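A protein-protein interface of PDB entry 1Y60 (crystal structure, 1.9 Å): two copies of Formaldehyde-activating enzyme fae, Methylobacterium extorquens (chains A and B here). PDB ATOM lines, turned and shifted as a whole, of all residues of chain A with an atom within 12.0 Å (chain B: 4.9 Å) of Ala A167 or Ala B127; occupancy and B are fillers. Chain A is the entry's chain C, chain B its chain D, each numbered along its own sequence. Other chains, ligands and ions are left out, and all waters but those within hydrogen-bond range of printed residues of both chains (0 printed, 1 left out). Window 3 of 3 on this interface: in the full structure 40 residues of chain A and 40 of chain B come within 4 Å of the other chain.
No position is printed for both chains.
Of the 7 pairs that touch across the chains among the printed residues, none has its exchanged pair printed and touching as well.
Of chain B, only Asp B126, Ala B127 and Gln B130 come within 4 Å of Ala A167.
Ala B127 touches just these residues of chain A: Ala A167 and Asn A168.
Of chain A, only Phe A165 comes within 4 Å of Pro B85.
No residue of chain A comes within 4 Å of Asp B125.
Of the printed residues of chain A, Gln B130 touches Ala A166 (3.7 Å), Ala A167 (2.8 Å) and Asn A168 (3.4 Å).
No residue of chain A comes within 4 Å of Lys B131.
Of the printed residues of chain B, Phe A165 touches Pro B85 (3.3 Å).
Printed residues of chain B within 4 Å of Ala A166: Gln B130 (3.7 Å).
Of the printed residues of chain B, Asn A168 touches Ala B127 (3.9 Å) and Gln B130 (3.4 Å).
Ala A161 touches none of the printed residues of chain B.
Thr A162 touches none of the printed residues of chain B.
The nearest residue of chain B that does not touch Ala A167 is Pro B85 (4.2 Å).
Among the printed residues, pairs that only touch across the chains: Phe A165 with Pro B85 (3.3 Å), Ala A167 with Asp B126 (3.4 Å), Ala A167 with Ala B127 (3.5 Å), Ala A166 with Gln B130 (3.7 Å) and Asn A168 with Ala B127 (3.9 Å).
OD2 of Asp B125 lies within hydrogen-bond range of N of Ala B127 (3.0 Å).
N of Ala A167 is in hydrogen-bond range of OE1 of Gln B130.
The backbone NH (N) of Asn A168 lies within hydrogen-bond range of the side-chain amide oxygen (OE1) of Gln B130.
Of the 8 printed residues of chain B, 4 touch a printed residue of chain A.
Printed residues of chain B that touch a printed residue of chain A: Pro B85, Asp B126, Ala B127 and Gln B130.
Hydrophobic or aromatic side chains of chain B within 4 Å of the printed part of chain A: Pro B85 and Ala B127.
Of the 8 printed residues of chain A, 4 touch a printed residue of chain B.
Among the printed residues, 7 pairs touch across the chains.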
ATOM      1  N   ALA A 161      -0.689   6.185  -7.663  1.00  0.00           N
ATOM      2  CA  ALA A 161       0.514   6.453  -6.874  1.00  0.00           C
ATOM      3  C   ALA A 161       0.990   7.881  -7.098  1.00  0.00           C
ATOM      4  O   ALA A 161       0.816   8.436  -8.180  1.00  0.00           O
ATOM      5  CB  ALA A 161       1.612   5.473  -7.246  1.00  0.00           C
ATOM      6  N   THR A 162       1.604   8.471  -6.080  1.00  0.00           N
ATOM      7  CA  THR A 162       2.090   9.843  -6.186  1.00  0.00           C
ATOM      8  C   THR A 162       3.571  10.004  -5.848  1.00  0.00           C
ATOM      9  O   THR A 162       3.976   9.862  -4.696  1.00  0.00           O
ATOM     10  CB  THR A 162       1.276  10.782  -5.267  1.00  0.00           C
ATOM     11  OG1 THR A 162      -0.115  10.696  -5.603  1.00  0.00           O
ATOM     12  CG2 THR A 162       1.735  12.219  -5.438  1.00  0.00           C
ATOM     13  N   HIS A 163       4.378  10.306  -6.859  1.00  0.00           N
ATOM     14  CA  HIS A 163       5.805  10.495  -6.644  1.00  0.00           C
ATOM     15  C   HIS A 163       5.964  11.937  -6.212  1.00  0.00           C
ATOM     16  O   HIS A 163       5.565  12.842  -6.930  1.00  0.00           O
ATOM     17  CB  HIS A 163       6.582  10.245  -7.934  1.00  0.00           C
ATOM     18  CG  HIS A 163       8.066  10.210  -7.742  1.00  0.00           C
ATOM     19  ND1 HIS A 163       8.911   9.527  -8.586  1.00  0.00           N
ATOM     20  CD2 HIS A 163       8.857  10.770  -6.800  1.00  0.00           C
ATOM     21  CE1 HIS A 163      10.158   9.667  -8.170  1.00  0.00           C
ATOM     22  NE2 HIS A 163      10.152  10.416  -7.087  1.00  0.00           N
ATOM     23  N   PRO A 164       6.544  12.176  -5.030  1.00  0.00           N
ATOM     24  CA  PRO A 164       6.727  13.542  -4.536  1.00  0.00           C
ATOM     25  C   PRO A 164       7.500  14.507  -5.432  1.00  0.00           C
ATOM     26  O   PRO A 164       7.296  15.722  -5.354  1.00  0.00           O
ATOM     27  CB  PRO A 164       7.431  13.325  -3.195  1.00  0.00           C
ATOM     28  CG  PRO A 164       8.234  12.079  -3.438  1.00  0.00           C
ATOM     29  CD  PRO A 164       7.204  11.209  -4.134  1.00  0.00           C
ATOM     30  N   PHE A 165       8.393  13.985  -6.268  1.00  0.00           N
ATOM     31  CA  PHE A 165       9.195  14.856  -7.126  1.00  0.00           C
ATOM     32  C   PHE A 165       8.785  14.851  -8.582  1.00  0.00           C
ATOM     33  O   PHE A 165       9.427  15.493  -9.411  1.00  0.00           O
ATOM     34  CB  PHE A 165      10.665  14.479  -7.009  1.00  0.00           C
ATOM     35  CG  PHE A 165      11.175  14.490  -5.602  1.00  0.00           C
ATOM     36  CD1 PHE A 165      11.058  15.633  -4.817  1.00  0.00           C
ATOM     37  CD2 PHE A 165      11.787  13.363  -5.059  1.00  0.00           C
ATOM     38  CE1 PHE A 165      11.546  15.656  -3.508  1.00  0.00           C
ATOM     39  CE2 PHE A 165      12.280  13.375  -3.748  1.00  0.00           C
ATOM     40  CZ  PHE A 165      12.159  14.524  -2.973  1.00  0.00           C
ATOM     41  N   ALA A 166       7.721  14.119  -8.895  1.00  0.00           N
ATOM     42  CA  ALA A 166       7.220  14.046 -10.261  1.00  0.00           C
ATOM     43  C   ALA A 166       6.807  15.449 -10.687  1.00  0.00           C
ATOM     44  O   ALA A 166       6.500  16.292  -9.846  1.00  0.00           O
ATOM     45  CB  ALA A 166       6.018  13.104 -10.328  1.00  0.00           C
ATOM     46  N   ALA A 167       6.824  15.716 -11.987  1.00  0.00           N
ATOM     47  CA  ALA A 167       6.399  17.021 -12.473  1.00  0.00           C
ATOM     48  C   ALA A 167       4.881  17.004 -12.330  1.00  0.00           C
ATOM     49  O   ALA A 167       4.286  17.807 -11.598  1.00  0.00           O
ATOM     50  CB  ALA A 167       6.780  17.193 -13.936  1.00  0.00           C
ATOM     51  N   ASN A 168       4.281  16.046 -13.035  1.00  0.00           N
ATOM     52  CA  ASN A 168       2.842  15.829 -13.054  1.00  0.00           C
ATOM     53  C   ASN A 168       2.504  14.757 -12.018  1.00  0.00           C
ATOM     54  O   ASN A 168       2.227  13.602 -12.412  1.00  0.00           O
ATOM     55  CB  ASN A 168       2.404  15.379 -14.463  1.00  0.00           C
ATOM     56  CG  ASN A 168       2.713  16.426 -15.546  1.00  0.00           C
ATOM     57  OD1 ASN A 168       2.006  17.426 -15.687  1.00  0.00           O
ATOM     58  ND2 ASN A 168       3.780  16.195 -16.305  1.00  0.00           N
ATOM     59  N   PRO B  85      10.959  13.848 -12.157  1.00  0.00           N
ATOM     60  CA  PRO B  85      10.249  13.710 -13.428  1.00  0.00           C
ATOM     61  C   PRO B  85      10.759  12.566 -14.295  1.00  0.00           C
ATOM     62  O   PRO B  85       9.965  11.778 -14.821  1.00  0.00           O
ATOM     63  CB  PRO B  85      10.443  15.076 -14.090  1.00  0.00           C
ATOM     64  CG  PRO B  85      11.687  15.617 -13.437  1.00  0.00           C
ATOM     65  CD  PRO B  85      11.494  15.212 -12.009  1.00  0.00           C
ATOM     66  N   ASP B 125      12.243  22.390 -17.832  1.00  0.00           N
ATOM     67  CA  ASP B 125      10.822  22.068 -17.752  1.00  0.00           C
ATOM     68  C   ASP B 125      10.557  20.615 -17.324  1.00  0.00           C
ATOM     69  O   ASP B 125      10.658  19.679 -18.134  1.00  0.00           O
ATOM     70  CB  ASP B 125      10.182  22.370 -19.108  1.00  0.00           C
ATOM     71  CG  ASP B 125       8.681  22.186 -19.118  1.00  0.00           C
ATOM     72  OD1 ASP B 125       8.050  22.638 -20.094  1.00  0.00           O
ATOM     73  OD2 ASP B 125       8.128  21.582 -18.182  1.00  0.00           O
ATOM     74  N   ASP B 126      10.185  20.446 -16.054  1.00  0.00           N
ATOM     75  CA  ASP B 126       9.915  19.128 -15.499  1.00  0.00           C
ATOM     76  C   ASP B 126       8.894  18.339 -16.285  1.00  0.00           C
ATOM     77  O   ASP B 126       9.062  17.129 -16.480  1.00  0.00           O
ATOM     78  CB  ASP B 126       9.458  19.230 -14.044  1.00  0.00           C
ATOM     79  CG  ASP B 126      10.578  19.662 -13.110  1.00  0.00           C
ATOM     80  OD1 ASP B 126      11.762  19.506 -13.459  1.00  0.00           O
ATOM     81  OD2 ASP B 126      10.280  20.149 -12.008  1.00  0.00           O
ATOM     82  N   ALA B 127       7.837  19.012 -16.736  1.00  0.00           N
ATOM     83  CA  ALA B 127       6.788  18.341 -17.491  1.00  0.00           C
ATOM     84  C   ALA B 127       7.354  17.688 -18.746  1.00  0.00           C
ATOM     85  O   ALA B 127       6.950  16.570 -19.111  1.00  0.00           O
ATOM     86  CB  ALA B 127       5.699  19.334 -17.871  1.00  0.00           C
ATOM     87  N   LYS B 128       8.274  18.394 -19.411  1.00  0.00           N
ATOM     88  CA  LYS B 128       8.879  17.872 -20.632  1.00  0.00           C
ATOM     89  C   LYS B 128       9.847  16.729 -20.344  1.00  0.00           C
ATOM     90  O   LYS B 128       9.853  15.721 -21.065  1.00  0.00           O
ATOM     91  CB  LYS B 128       9.597  18.982 -21.393  1.00  0.00           C
ATOM     92  CG  LYS B 128       8.658  19.964 -22.067  1.00  0.00           C
ATOM     93  CD  LYS B 128       9.438  21.046 -22.765  1.00  0.00           C
ATOM     94  CE  LYS B 128       8.521  22.081 -23.396  1.00  0.00           C
ATOM     95  NZ  LYS B 128       9.318  23.014 -24.240  1.00  0.00           N
ATOM     96  N   ILE B 129      10.659  16.900 -19.304  1.00  0.00           N
ATOM     97  CA  ILE B 129      11.618  15.873 -18.898  1.00  0.00           C
ATOM     98  C   ILE B 129      10.835  14.583 -18.653  1.00  0.00           C
ATOM     99  O   ILE B 129      11.157  13.513 -19.185  1.00  0.00           O
ATOM    100  CB  ILE B 129      12.340  16.274 -17.595  1.00  0.00           C
ATOM    101  CG1 ILE B 129      13.216  17.507 -17.851  1.00  0.00           C
ATOM    102  CG2 ILE B 129      13.154  15.107 -17.075  1.00  0.00           C
ATOM    103  CD1 ILE B 129      13.859  18.066 -16.609  1.00  0.00           C
ATOM    104  N   GLN B 130       9.776  14.706 -17.868  1.00  0.00           N
ATOM    105  CA  GLN B 130       8.931  13.567 -17.556  1.00  0.00           C
ATOM    106  C   GLN B 130       8.286  12.944 -18.794  1.00  0.00           C
ATOM    107  O   GLN B 130       8.306  11.716 -18.965  1.00  0.00           O
ATOM    108  CB  GLN B 130       7.854  13.995 -16.569  1.00  0.00           C
ATOM    109  CG  GLN B 130       6.950  12.868 -16.126  1.00  0.00           C
ATOM    110  CD  GLN B 130       6.104  13.243 -14.947  1.00  0.00           C
ATOM    111  OE1 GLN B 130       6.617  13.745 -13.948  1.00  0.00           O
ATOM    112  NE2 GLN B 130       4.789  12.993 -15.041  1.00  0.00           N
ATOM    113  N   LYS B 131       7.725  13.777 -19.669  1.00  0.00           N
ATOM    114  CA  LYS B 131       7.070  13.263 -20.868  1.00  0.00           C
ATOM    115  C   LYS B 131       8.008  12.647 -21.889  1.00  0.00           C
ATOM    116  O   LYS B 131       7.737  11.566 -22.433  1.00  0.00           O
ATOM    117  CB  LYS B 131       6.262  14.365 -21.562  1.00  0.00           C
ATOM    118  CG  LYS B 131       5.582  13.892 -22.832  1.00  0.00           C
ATOM    119  CD  LYS B 131       4.755  14.985 -23.476  1.00  0.00           C
ATOM    120  CE  LYS B 131       4.003  14.456 -24.692  1.00  0.00           C
ATOM    121  NZ  LYS B 131       3.177  15.516 -25.329  1.00  0.00           N
